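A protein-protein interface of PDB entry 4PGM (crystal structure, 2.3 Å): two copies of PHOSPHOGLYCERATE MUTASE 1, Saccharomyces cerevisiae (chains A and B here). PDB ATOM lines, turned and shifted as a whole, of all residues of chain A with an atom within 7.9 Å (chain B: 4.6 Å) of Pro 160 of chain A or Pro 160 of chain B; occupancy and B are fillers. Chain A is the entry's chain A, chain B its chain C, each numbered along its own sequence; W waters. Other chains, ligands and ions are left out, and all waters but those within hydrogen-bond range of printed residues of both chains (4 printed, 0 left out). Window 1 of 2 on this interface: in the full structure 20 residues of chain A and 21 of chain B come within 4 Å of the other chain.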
ATOM      1  N   SER A  81     -17.902   0.443   3.475  1.00  0.00           N
ATOM      2  CA  SER A  81     -18.377   0.086   4.803  1.00  0.00           C
ATOM      3  C   SER A  81     -18.410   1.272   5.755  1.00  0.00           C
ATOM      4  O   SER A  81     -17.483   2.072   5.801  1.00  0.00           O
ATOM      5  CB  SER A  81     -17.431  -0.979   5.400  1.00  0.00           C
ATOM      6  OG  SER A  81     -17.797  -1.318   6.726  1.00  0.00           O
ATOM      7  N   TRP A  82     -19.455   1.337   6.564  1.00  0.00           N
ATOM      8  CA  TRP A  82     -19.579   2.371   7.582  1.00  0.00           C
ATOM      9  C   TRP A  82     -18.383   2.205   8.538  1.00  0.00           C
ATOM     10  O   TRP A  82     -17.798   3.177   8.997  1.00  0.00           O
ATOM     11  CB  TRP A  82     -20.897   2.221   8.365  1.00  0.00           C
ATOM     12  CG  TRP A  82     -20.955   1.081   9.351  1.00  0.00           C
ATOM     13  CD1 TRP A  82     -21.354  -0.197   9.103  1.00  0.00           C
ATOM     14  CD2 TRP A  82     -20.698   1.149  10.773  1.00  0.00           C
ATOM     15  NE1 TRP A  82     -21.384  -0.931  10.280  1.00  0.00           N
ATOM     16  CE2 TRP A  82     -20.985  -0.126  11.316  1.00  0.00           C
ATOM     17  CE3 TRP A  82     -20.269   2.170  11.637  1.00  0.00           C
ATOM     18  CZ2 TRP A  82     -20.849  -0.409  12.687  1.00  0.00           C
ATOM     19  CZ3 TRP A  82     -20.138   1.888  12.997  1.00  0.00           C
ATOM     20  CH2 TRP A  82     -20.429   0.606  13.506  1.00  0.00           C
ATOM     21  N   ARG A  83     -17.989   0.966   8.797  1.00  0.00           N
ATOM     22  CA  ARG A  83     -16.878   0.697   9.692  1.00  0.00           C
ATOM     23  C   ARG A  83     -15.583   1.423   9.379  1.00  0.00           C
ATOM     24  O   ARG A  83     -14.672   1.389  10.197  1.00  0.00           O
ATOM     25  CB  ARG A  83     -16.631  -0.808   9.784  1.00  0.00           C
ATOM     26  CG  ARG A  83     -17.714  -1.472  10.553  1.00  0.00           C
ATOM     27  CD  ARG A  83     -17.518  -2.972  10.755  1.00  0.00           C
ATOM     28  NE  ARG A  83     -18.793  -3.479  11.253  1.00  0.00           N
ATOM     29  CZ  ARG A  83     -19.125  -3.602  12.542  1.00  0.00           C
ATOM     30  NH1 ARG A  83     -18.252  -3.275  13.494  1.00  0.00           N
ATOM     31  NH2 ARG A  83     -20.374  -3.942  12.871  1.00  0.00           N
ATOM     32  N   VAL A 140     -27.920  -1.678   8.190  1.00  0.00           N
ATOM     33  CA  VAL A 140     -27.058  -1.948   9.339  1.00  0.00           C
ATOM     34  C   VAL A 140     -27.961  -1.899  10.578  1.00  0.00           C
ATOM     35  O   VAL A 140     -28.980  -1.196  10.590  1.00  0.00           O
ATOM     36  CB  VAL A 140     -25.934  -0.881   9.504  1.00  0.00           C
ATOM     37  CG1 VAL A 140     -25.192  -1.090  10.817  1.00  0.00           C
ATOM     38  CG2 VAL A 140     -24.944  -0.962   8.363  1.00  0.00           C
ATOM     39  N   ASP A 141     -27.645  -2.735  11.558  1.00  0.00           N
ATOM     40  CA  ASP A 141     -28.383  -2.788  12.826  1.00  0.00           C
ATOM     41  C   ASP A 141     -28.541  -1.336  13.392  1.00  0.00           C
ATOM     42  O   ASP A 141     -27.547  -0.676  13.714  1.00  0.00           O
ATOM     43  CB  ASP A 141     -27.545  -3.670  13.774  1.00  0.00           C
ATOM     44  CG  ASP A 141     -28.146  -3.842  15.145  1.00  0.00           C
ATOM     45  OD1 ASP A 141     -29.299  -3.439  15.423  1.00  0.00           O
ATOM     46  OD2 ASP A 141     -27.426  -4.416  15.974  1.00  0.00           O
ATOM     47  N   VAL A 144     -26.370  -0.195  16.521  1.00  0.00           N
ATOM     48  CA  VAL A 144     -24.918  -0.086  16.533  1.00  0.00           C
ATOM     49  C   VAL A 144     -24.398   1.283  16.126  1.00  0.00           C
ATOM     50  O   VAL A 144     -23.282   1.652  16.498  1.00  0.00           O
ATOM     51  CB  VAL A 144     -24.246  -1.169  15.639  1.00  0.00           C
ATOM     52  CG1 VAL A 144     -24.330  -0.802  14.140  1.00  0.00           C
ATOM     53  CG2 VAL A 144     -22.797  -1.357  16.052  1.00  0.00           C
ATOM     54  N   LEU A 153     -13.578   3.848  20.398  1.00  0.00           N
ATOM     55  CA  LEU A 153     -14.806   3.335  19.812  1.00  0.00           C
ATOM     56  C   LEU A 153     -14.629   3.080  18.313  1.00  0.00           C
ATOM     57  O   LEU A 153     -15.045   2.046  17.800  1.00  0.00           O
ATOM     58  CB  LEU A 153     -15.940   4.332  20.073  1.00  0.00           C
ATOM     59  CG  LEU A 153     -16.895   4.049  21.236  1.00  0.00           C
ATOM     60  CD1 LEU A 153     -16.174   3.370  22.333  1.00  0.00           C
ATOM     61  CD2 LEU A 153     -17.584   5.318  21.741  1.00  0.00           C
ATOM     62  N   VAL A 154     -13.966   3.997  17.620  1.00  0.00           N
ATOM     63  CA  VAL A 154     -13.736   3.863  16.190  1.00  0.00           C
ATOM     64  C   VAL A 154     -12.922   2.617  15.908  1.00  0.00           C
ATOM     65  O   VAL A 154     -13.265   1.835  15.026  1.00  0.00           O
ATOM     66  CB  VAL A 154     -13.007   5.118  15.591  1.00  0.00           C
ATOM     67  CG1 VAL A 154     -12.472   4.829  14.152  1.00  0.00           C
ATOM     68  CG2 VAL A 154     -13.947   6.308  15.587  1.00  0.00           C
ATOM     69  N   ILE A 155     -11.831   2.447  16.642  1.00  0.00           N
ATOM     70  CA  ILE A 155     -10.950   1.279  16.470  1.00  0.00           C
ATOM     71  C   ILE A 155     -11.742  -0.002  16.739  1.00  0.00           C
ATOM     72  O   ILE A 155     -11.515  -1.019  16.090  1.00  0.00           O
ATOM     73  CB  ILE A 155      -9.732   1.347  17.448  1.00  0.00           C
ATOM     74  CG1 ILE A 155      -8.917   2.616  17.171  1.00  0.00           C
ATOM     75  CG2 ILE A 155      -8.848   0.094  17.331  1.00  0.00           C
ATOM     76  CD1 ILE A 155      -7.800   2.838  18.166  1.00  0.00           C
ATOM     77  N   ASP A 156     -12.734   0.101  17.622  1.00  0.00           N
ATOM     78  CA  ASP A 156     -13.576  -1.020  18.006  1.00  0.00           C
ATOM     79  C   ASP A 156     -14.563  -1.502  16.946  1.00  0.00           C
ATOM     80  O   ASP A 156     -14.772  -2.706  16.794  1.00  0.00           O
ATOM     81  CB  ASP A 156     -14.333  -0.686  19.295  1.00  0.00           C
ATOM     82  CG  ASP A 156     -13.473  -0.830  20.551  1.00  0.00           C
ATOM     83  OD1 ASP A 156     -12.273  -1.189  20.473  1.00  0.00           O
ATOM     84  OD2 ASP A 156     -14.021  -0.586  21.638  1.00  0.00           O
ATOM     85  N   ARG A 157     -15.235  -0.566  16.283  1.00  0.00           N
ATOM     86  CA  ARG A 157     -16.195  -0.934  15.254  1.00  0.00           C
ATOM     87  C   ARG A 157     -15.524  -1.130  13.907  1.00  0.00           C
ATOM     88  O   ARG A 157     -16.100  -1.717  13.002  1.00  0.00           O
ATOM     89  CB  ARG A 157     -17.369   0.055  15.188  1.00  0.00           C
ATOM     90  CG  ARG A 157     -16.992   1.503  15.111  1.00  0.00           C
ATOM     91  CD  ARG A 157     -16.668   1.960  13.693  1.00  0.00           C
ATOM     92  NE  ARG A 157     -16.770   3.417  13.617  1.00  0.00           N
ATOM     93  CZ  ARG A 157     -16.173   4.174  12.709  1.00  0.00           C
ATOM     94  NH1 ARG A 157     -15.419   3.635  11.773  1.00  0.00           N
ATOM     95  NH2 ARG A 157     -16.285   5.485  12.795  1.00  0.00           N
ATOM     96  N   LEU A 158     -14.273  -0.710  13.815  1.00  0.00           N
ATOM     97  CA  LEU A 158     -13.517  -0.871  12.594  1.00  0.00           C
ATOM     98  C   LEU A 158     -12.803  -2.212  12.567  1.00  0.00           C
ATOM     99  O   LEU A 158     -12.817  -2.903  11.550  1.00  0.00           O
ATOM    100  CB  LEU A 158     -12.493   0.245  12.450  1.00  0.00           C
ATOM    101  CG  LEU A 158     -11.501   0.140  11.284  1.00  0.00           C
ATOM    102  CD1 LEU A 158     -11.401   1.479  10.544  1.00  0.00           C
ATOM    103  CD2 LEU A 158     -10.149  -0.316  11.786  1.00  0.00           C
ATOM    104  N   LEU A 159     -12.217  -2.610  13.690  1.00  0.00           N
ATOM    105  CA  LEU A 159     -11.459  -3.867  13.739  1.00  0.00           C
ATOM    106  C   LEU A 159     -12.078  -5.112  13.111  1.00  0.00           C
ATOM    107  O   LEU A 159     -11.395  -5.840  12.389  1.00  0.00           O
ATOM    108  CB  LEU A 159     -10.894  -4.158  15.144  1.00  0.00           C
ATOM    109  CG  LEU A 159      -9.505  -3.561  15.418  1.00  0.00           C
ATOM    110  CD1 LEU A 159      -8.930  -4.050  16.737  1.00  0.00           C
ATOM    111  CD2 LEU A 159      -8.565  -3.921  14.285  1.00  0.00           C
ATOM    112  N   PRO A 160     -13.368  -5.384  13.359  1.00  0.00           N
ATOM    113  CA  PRO A 160     -13.995  -6.579  12.768  1.00  0.00           C
ATOM    114  C   PRO A 160     -14.121  -6.624  11.235  1.00  0.00           C
ATOM    115  O   PRO A 160     -14.212  -7.713  10.628  1.00  0.00           O
ATOM    116  CB  PRO A 160     -15.359  -6.650  13.464  1.00  0.00           C
ATOM    117  CG  PRO A 160     -15.582  -5.239  13.975  1.00  0.00           C
ATOM    118  CD  PRO A 160     -14.215  -4.813  14.413  1.00  0.00           C
ATOM    119  N   TYR A 161     -14.124  -5.443  10.623  1.00  0.00           N
ATOM    120  CA  TYR A 161     -14.218  -5.337   9.183  1.00  0.00           C
ATOM    121  C   TYR A 161     -12.840  -5.695   8.678  1.00  0.00           C
ATOM    122  O   TYR A 161     -12.680  -6.529   7.766  1.00  0.00           O
ATOM    123  CB  TYR A 161     -14.592  -3.903   8.752  1.00  0.00           C
ATOM    124  CG  TYR A 161     -14.913  -3.774   7.279  1.00  0.00           C
ATOM    125  CD1 TYR A 161     -16.067  -4.362   6.735  1.00  0.00           C
ATOM    126  CD2 TYR A 161     -14.051  -3.107   6.419  1.00  0.00           C
ATOM    127  CE1 TYR A 161     -16.346  -4.285   5.355  1.00  0.00           C
ATOM    128  CE2 TYR A 161     -14.316  -3.022   5.034  1.00  0.00           C
ATOM    129  CZ  TYR A 161     -15.462  -3.614   4.514  1.00  0.00           C
ATOM    130  OH  TYR A 161     -15.710  -3.529   3.169  1.00  0.00           O
ATOM    131  N   TRP A 162     -11.833  -5.113   9.322  1.00  0.00           N
ATOM    132  CA  TRP A 162     -10.441  -5.366   8.959  1.00  0.00           C
ATOM    133  C   TRP A 162     -10.118  -6.854   9.074  1.00  0.00           C
ATOM    134  O   TRP A 162      -9.512  -7.446   8.178  1.00  0.00           O
ATOM    135  CB  TRP A 162      -9.519  -4.569   9.898  1.00  0.00           C
ATOM    136  CG  TRP A 162      -8.093  -5.098   9.991  1.00  0.00           C
ATOM    137  CD1 TRP A 162      -7.546  -5.836  11.015  1.00  0.00           C
ATOM    138  CD2 TRP A 162      -7.054  -4.933   9.022  1.00  0.00           C
ATOM    139  NE1 TRP A 162      -6.228  -6.143  10.735  1.00  0.00           N
ATOM    140  CE2 TRP A 162      -5.897  -5.597   9.521  1.00  0.00           C
ATOM    141  CE3 TRP A 162      -6.980  -4.287   7.776  1.00  0.00           C
ATOM    142  CZ2 TRP A 162      -4.700  -5.633   8.826  1.00  0.00           C
ATOM    143  CZ3 TRP A 162      -5.796  -4.328   7.087  1.00  0.00           C
ATOM    144  CH2 TRP A 162      -4.667  -4.995   7.612  1.00  0.00           C
ATOM    145  N   GLN A 163     -10.506  -7.432  10.214  1.00  0.00           N
ATOM    146  CA  GLN A 163     -10.276  -8.835  10.575  1.00  0.00           C
ATOM    147  C   GLN A 163     -10.876  -9.914   9.667  1.00  0.00           C
ATOM    148  O   GLN A 163     -10.253 -10.958   9.440  1.00  0.00           O
ATOM    149  CB  GLN A 163     -10.783  -9.076  12.004  1.00  0.00           C
ATOM    150  CG  GLN A 163     -10.025  -8.327  13.097  1.00  0.00           C
ATOM    151  CD  GLN A 163     -10.787  -8.298  14.417  1.00  0.00           C
ATOM    152  OE1 GLN A 163     -11.954  -8.693  14.487  1.00  0.00           O
ATOM    153  NE2 GLN A 163     -10.130  -7.805  15.467  1.00  0.00           N
ATOM    154  N   ASP A 164     -12.104  -9.682   9.205  1.00  0.00           N
ATOM    155  CA  ASP A 164     -12.804 -10.637   8.356  1.00  0.00           C
ATOM    156  C   ASP A 164     -12.761 -10.359   6.857  1.00  0.00           C
ATOM    157  O   ASP A 164     -12.598 -11.275   6.033  1.00  0.00           O
ATOM    158  CB  ASP A 164     -14.275 -10.650   8.737  1.00  0.00           C
ATOM    159  CG  ASP A 164     -14.550 -11.375  10.025  1.00  0.00           C
ATOM    160  OD1 ASP A 164     -13.613 -11.879  10.657  1.00  0.00           O
ATOM    161  OD2 ASP A 164     -15.739 -11.461  10.394  1.00  0.00           O
ATOM    162  N   VAL A 165     -13.041  -9.102   6.520  1.00  0.00           N
ATOM    163  CA  VAL A 165     -13.120  -8.658   5.151  1.00  0.00           C
ATOM    164  C   VAL A 165     -11.824  -8.231   4.501  1.00  0.00           C
ATOM    165  O   VAL A 165     -11.401  -8.840   3.531  1.00  0.00           O
ATOM    166  CB  VAL A 165     -14.137  -7.518   5.019  1.00  0.00           C
ATOM    167  CG1 VAL A 165     -14.440  -7.262   3.558  1.00  0.00           C
ATOM    168  CG2 VAL A 165     -15.410  -7.865   5.741  1.00  0.00           C
ATOM    169  N   ILE A 166     -11.186  -7.189   5.016  1.00  0.00           N
ATOM    170  CA  ILE A 166      -9.971  -6.707   4.376  1.00  0.00           C
ATOM    171  C   ILE A 166      -8.885  -7.750   4.491  1.00  0.00           C
ATOM    172  O   ILE A 166      -8.173  -8.001   3.519  1.00  0.00           O
ATOM    173  CB  ILE A 166      -9.525  -5.332   4.944  1.00  0.00           C
ATOM    174  CG1 ILE A 166     -10.708  -4.364   4.941  1.00  0.00           C
ATOM    175  CG2 ILE A 166      -8.434  -4.744   4.082  1.00  0.00           C
ATOM    176  CD1 ILE A 166     -10.431  -3.058   5.609  1.00  0.00           C
ATOM    177  N   ALA A 167      -8.825  -8.411   5.653  1.00  0.00           N
ATOM    178  CA  ALA A 167      -7.865  -9.483   5.915  1.00  0.00           C
ATOM    179  C   ALA A 167      -7.897 -10.594   4.851  1.00  0.00           C
ATOM    180  O   ALA A 167      -6.852 -11.107   4.475  1.00  0.00           O
ATOM    181  CB  ALA A 167      -8.128 -10.096   7.263  1.00  0.00           C
ATOM    182  N   ARG B  83     -17.248 -16.394  13.473  1.00  0.00           N
ATOM    183  CA  ARG B  83     -17.922 -15.596  14.502  1.00  0.00           C
ATOM    184  C   ARG B  83     -19.145 -16.199  15.181  1.00  0.00           C
ATOM    185  O   ARG B  83     -19.526 -15.718  16.252  1.00  0.00           O
ATOM    186  CB  ARG B  83     -18.264 -14.216  13.969  1.00  0.00           C
ATOM    187  CG  ARG B  83     -17.031 -13.434  13.735  1.00  0.00           C
ATOM    188  CD  ARG B  83     -17.244 -12.036  13.282  1.00  0.00           C
ATOM    189  NE  ARG B  83     -15.927 -11.504  12.953  1.00  0.00           N
ATOM    190  CZ  ARG B  83     -15.183 -10.726  13.737  1.00  0.00           C
ATOM    191  NH1 ARG B  83     -15.620 -10.363  14.933  1.00  0.00           N
ATOM    192  NH2 ARG B  83     -13.966 -10.366  13.339  1.00  0.00           N
ATOM    193  N   ASP B 156     -18.312 -10.367  21.841  1.00  0.00           N
ATOM    194  CA  ASP B 156     -17.556  -9.318  21.146  1.00  0.00           C
ATOM    195  C   ASP B 156     -17.388  -9.633  19.663  1.00  0.00           C
ATOM    196  O   ASP B 156     -17.641  -8.796  18.809  1.00  0.00           O
ATOM    197  CB  ASP B 156     -16.149  -9.146  21.743  1.00  0.00           C
ATOM    198  CG  ASP B 156     -16.159  -8.678  23.184  1.00  0.00           C
ATOM    199  OD1 ASP B 156     -17.209  -8.222  23.694  1.00  0.00           O
ATOM    200  OD2 ASP B 156     -15.083  -8.776  23.807  1.00  0.00           O
ATOM    201  N   ARG B 157     -16.909 -10.840  19.384  1.00  0.00           N
ATOM    202  CA  ARG B 157     -16.695 -11.299  18.016  1.00  0.00           C
ATOM    203  C   ARG B 157     -17.985 -11.677  17.267  1.00  0.00           C
ATOM    204  O   ARG B 157     -18.021 -11.647  16.044  1.00  0.00           O
ATOM    205  CB  ARG B 157     -15.721 -12.481  18.008  1.00  0.00           C
ATOM    206  CG  ARG B 157     -15.842 -13.350  19.238  1.00  0.00           C
ATOM    207  CD  ARG B 157     -15.713 -14.826  18.926  1.00  0.00           C
ATOM    208  NE  ARG B 157     -16.972 -15.440  18.502  1.00  0.00           N
ATOM    209  CZ  ARG B 157     -17.305 -16.708  18.745  1.00  0.00           C
ATOM    210  NH1 ARG B 157     -16.467 -17.496  19.422  1.00  0.00           N
ATOM    211  NH2 ARG B 157     -18.453 -17.193  18.281  1.00  0.00           N
ATOM    212  N   LEU B 158     -19.043 -12.019  17.989  1.00  0.00           N
ATOM    213  CA  LEU B 158     -20.291 -12.399  17.340  1.00  0.00           C
ATOM    214  C   LEU B 158     -21.085 -11.203  16.870  1.00  0.00           C
ATOM    215  O   LEU B 158     -21.684 -11.243  15.804  1.00  0.00           O
ATOM    216  CB  LEU B 158     -21.158 -13.245  18.283  1.00  0.00           C
ATOM    217  CG  LEU B 158     -22.524 -13.830  17.892  1.00  0.00           C
ATOM    218  CD1 LEU B 158     -22.902 -14.921  18.877  1.00  0.00           C
ATOM    219  CD2 LEU B 158     -23.615 -12.771  17.884  1.00  0.00           C
ATOM    220  N   LEU B 159     -21.114 -10.149  17.672  1.00  0.00           N
ATOM    221  CA  LEU B 159     -21.912  -8.961  17.343  1.00  0.00           C
ATOM    222  C   LEU B 159     -21.678  -8.278  15.978  1.00  0.00           C
ATOM    223  O   LEU B 159     -22.632  -7.896  15.297  1.00  0.00           O
ATOM    224  CB  LEU B 159     -21.878  -7.944  18.500  1.00  0.00           C
ATOM    225  CG  LEU B 159     -22.588  -8.442  19.759  1.00  0.00           C
ATOM    226  CD1 LEU B 159     -22.652  -7.358  20.812  1.00  0.00           C
ATOM    227  CD2 LEU B 159     -23.985  -8.908  19.427  1.00  0.00           C
ATOM    228  N   PRO B 160     -20.424  -8.124  15.551  1.00  0.00           N
ATOM    229  CA  PRO B 160     -20.227  -7.479  14.252  1.00  0.00           C
ATOM    230  C   PRO B 160     -20.906  -8.210  13.112  1.00  0.00           C
ATOM    231  O   PRO B 160     -21.518  -7.586  12.249  1.00  0.00           O
ATOM    232  CB  PRO B 160     -18.720  -7.491  14.095  1.00  0.00           C
ATOM    233  CG  PRO B 160     -18.268  -7.338  15.535  1.00  0.00           C
ATOM    234  CD  PRO B 160     -19.144  -8.312  16.247  1.00  0.00           C
ATOM    235  N   TYR B 161     -20.810  -9.538  13.145  1.00  0.00           N
ATOM    236  CA  TYR B 161     -21.390 -10.396  12.122  1.00  0.00           C
ATOM    237  C   TYR B 161     -22.890 -10.219  12.115  1.00  0.00           C
ATOM    238  O   TYR B 161     -23.528 -10.174  11.056  1.00  0.00           O
ATOM    239  CB  TYR B 161     -21.046 -11.863  12.376  1.00  0.00           C
ATOM    240  CG  TYR B 161     -21.313 -12.721  11.175  1.00  0.00           C
ATOM    241  CD1 TYR B 161     -20.523 -12.579  10.011  1.00  0.00           C
ATOM    242  CD2 TYR B 161     -22.345 -13.664  11.171  1.00  0.00           C
ATOM    243  CE1 TYR B 161     -20.750 -13.354   8.884  1.00  0.00           C
ATOM    244  CE2 TYR B 161     -22.587 -14.457  10.020  1.00  0.00           C
ATOM    245  CZ  TYR B 161     -21.781 -14.294   8.892  1.00  0.00           C
ATOM    246  OH  TYR B 161     -21.960 -15.083   7.784  1.00  0.00           O
ATOM    247  N   TRP B 162     -23.457 -10.112  13.301  1.00  0.00           N
ATOM    248  CA  TRP B 162     -24.889  -9.907  13.427  1.00  0.00           C
ATOM    249  C   TRP B 162     -25.272  -8.491  12.949  1.00  0.00           C
ATOM    250  O   TRP B 162     -26.322  -8.296  12.321  1.00  0.00           O
ATOM    251  CB  TRP B 162     -25.289 -10.097  14.899  1.00  0.00           C
ATOM    252  CG  TRP B 162     -26.638  -9.529  15.251  1.00  0.00           C
ATOM    253  CD1 TRP B 162     -26.902  -8.292  15.771  1.00  0.00           C
ATOM    254  CD2 TRP B 162     -27.904 -10.152  15.032  1.00  0.00           C
ATOM    255  NE1 TRP B 162     -28.261  -8.098  15.869  1.00  0.00           N
ATOM    256  CE2 TRP B 162     -28.900  -9.225  15.422  1.00  0.00           C
ATOM    257  CE3 TRP B 162     -28.303 -11.400  14.535  1.00  0.00           C
ATOM    258  CZ2 TRP B 162     -30.250  -9.508  15.331  1.00  0.00           C
ATOM    259  CZ3 TRP B 162     -29.639 -11.674  14.440  1.00  0.00           C
ATOM    260  CH2 TRP B 162     -30.601 -10.741  14.836  1.00  0.00           C
ATOM    261  N   GLN B 163     -24.419  -7.515  13.272  1.00  0.00           N
ATOM    262  CA  GLN B 163     -24.643  -6.107  12.957  1.00  0.00           C
ATOM    263  C   GLN B 163     -24.609  -5.754  11.484  1.00  0.00           C
ATOM    264  O   GLN B 163     -25.474  -5.028  11.001  1.00  0.00           O
ATOM    265  CB  GLN B 163     -23.661  -5.224  13.741  1.00  0.00           C
ATOM    266  CG  GLN B 163     -24.017  -5.105  15.228  1.00  0.00           C
ATOM    267  CD  GLN B 163     -22.832  -4.736  16.132  1.00  0.00           C
ATOM    268  OE1 GLN B 163     -21.672  -4.632  15.684  1.00  0.00           O
ATOM    269  NE2 GLN B 163     -23.120  -4.535  17.414  1.00  0.00           N
ATOM    270  N   ASP B 164     -23.610  -6.267  10.782  1.00  0.00           N
ATOM    271  CA  ASP B 164     -23.444  -6.011   9.367  1.00  0.00           C
ATOM    272  C   ASP B 164     -24.122  -7.043   8.464  1.00  0.00           C
ATOM    273  O   ASP B 164     -25.003  -6.709   7.658  1.00  0.00           O
ATOM    274  CB  ASP B 164     -21.951  -5.983   9.033  1.00  0.00           C
ATOM    275  CG  ASP B 164     -21.256  -4.721   9.515  1.00  0.00           C
ATOM    276  OD1 ASP B 164     -21.787  -4.035  10.413  1.00  0.00           O
ATOM    277  OD2 ASP B 164     -20.160  -4.428   8.995  1.00  0.00           O
ATOM    278  N   VAL B 165     -23.659  -8.291   8.582  1.00  0.00           N
ATOM    279  CA  VAL B 165     -24.134  -9.414   7.779  1.00  0.00           C
ATOM    280  C   VAL B 165     -25.539  -9.963   8.069  1.00  0.00           C
ATOM    281  O   VAL B 165     -26.422  -9.844   7.217  1.00  0.00           O
ATOM    282  CB  VAL B 165     -23.074 -10.530   7.763  1.00  0.00           C
ATOM    283  CG1 VAL B 165     -23.215 -11.418   6.531  1.00  0.00           C
ATOM    284  CG2 VAL B 165     -21.699  -9.909   7.764  1.00  0.00           C
HETATM  285  O   HOH W   1     -29.244  -5.694  17.876  1.00  0.00           O
HETATM  286  O   HOH W   2     -19.260  -3.497  16.500  1.00  0.00           O
HETATM  287  O   HOH W   3     -25.945  -4.384  18.315  1.00  0.00           O
HETATM  288  O   HOH W   4     -19.911  -3.093   6.832  1.00  0.00           O
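CA of Pro 160 of chain B touches NH2 of Arg 83 of chain A, 3.8 Å away.
O of Gln 163 of chain B touches CA of Val 140 of chain A, 3.8 Å away.
Asp 141 of chain A touches Trp 162 of chain B (OD2 to NE1, 3.8 Å).
CG2 of Val 144 of chain A touches CD of Gln 163 of chain B (3.4 Å).
Arg 83 of chain B touches Pro 160 of chain A.
Pro 160 of chain A touches Pro 160 of chain B.
OD1 of Asp 164 of chain B is in hydrogen-bond range of NE1 of Trp 82 of chain A (3.1 Å).
The guanidinium group of Arg 83 of chain A is in hydrogen-bond range of the side-chain amide oxygen of Gln 163 of chain B (3.2 Å).
The guanidinium group (NE) of Arg 83 of chain A lies within salt-bridge range of the side-chain carboxylate (OD2) of Asp 164 of chain B.
The backbone carbonyl oxygen (O) of Gln 163 of chain B is in hydrogen-bond range of the backbone NH (N) of Asp 141 of chain A (3.2 Å).
The side-chain amide oxygen (OE1) of Gln 163 of chain A sits at hydrogen-bond distance from the guanidinium group (NH2) of Arg 83 of chain B, 2.9 Å away.
The guanidinium group (NE) of Arg 83 of chain B lies within salt-bridge range of the side-chain carboxylate (OD2) of Asp 164 of chain A, 2.6 Å away.
Water W4 bridges the side-chain carboxylate (OD2) of Asp 164 of chain B and the side-chain hydroxyl (OG) of Ser 81 of chain A.
Water W3 bridges the side-chain carboxylate (OD2) of Asp 141 of chain A and the side-chain amide nitrogen (NE2) of Gln 163 of chain B.
Water W2 bridges the side-chain amide oxygen of Gln 163 of chain B (2.8 Å) and the guanidinium group of Arg 83 of chain A (3.2 Å).
Water W1 lies within hydrogen-bond range of OD2 of Asp 141 of chain A and NE1 of Trp 162 of chain B.
Arg 83 of chain A touches Pro 160 of chain B, and with the chains exchanged Pro 160 of chain A touches Arg 83 of chain B.
Arg 83 of chain A touches Gln 163 of chain B, and with the chains exchanged Gln 163 of chain A touches Arg 83 of chain B.
Arg 83 of chain A touches Asp 164 of chain B, and with the chains exchanged Asp 164 of chain A touches Arg 83 of chain B.
Pro 160 of chain B touches its own counterpart, Pro 160 of chain A.
11 positions are printed for both chains.
Of the printed residues of chain B, Val 140 of chain A touches Gln 163.
Pro 160 of chain A touches just these residues of chain B: Arg 83 and Pro 160.
Of the printed residues of chain A, Arg 83 of chain B touches Pro 160 (3.8 Å), Gln 163 (2.9 Å) and Asp 164 (2.6 Å).
Leu 159 of chain B touches none of the printed residues of chain A.
Of chain A, only Arg 83 and Pro 160 come within 4 Å of Pro 160 of chain B.
Of the printed residues of chain A, Gln 163 of chain B touches Arg 83 (3.2 Å), Val 140 (3.8 Å), Asp 141 (3.2 Å) and Val 144 (3.4 Å).
Of the printed residues of chain A, Asp 164 of chain B touches Trp 82 (3.1 Å) and Arg 83 (2.8 Å).
The nearest printed residue of chain B that does not touch Pro 160 of chain A is Tyr 161 of chain B (6.2 Å).
The nearest residue of chain A that does not touch Pro 160 of chain B is Asp 156 of chain A (5.9 Å).
Of the 11 printed residues of chain B, 5 touch a printed residue of chain A.
Printed residues of chain B that touch a printed residue of chain A: Arg 83, Pro 160, Trp 162, Gln 163 and Asp 164.
Hydrophobic or aromatic side chains of chain B within 4 Å of the printed part of chain A: Pro 160 and Trp 162.
Among the printed residues, 12 pairs touch across the chains.
OG of Ser 81 of chain A lies close to N of Arg 83 of chain A (3.1 Å).
The guanidinium group (NH1) of Arg 83 of chain A sits at hydrogen-bond distance from the backbone carbonyl oxygen (O) of Arg 157 of chain A (2.7 Å).
NH2 of Arg 157 of chain B sits at hydrogen-bond distance from O of Arg 83 of chain B (2.7 Å).
The side-chain amide oxygen of Gln 163 of chain B lies close to the backbone carbonyl oxygen of Leu 159 of chain B (3.4 Å).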
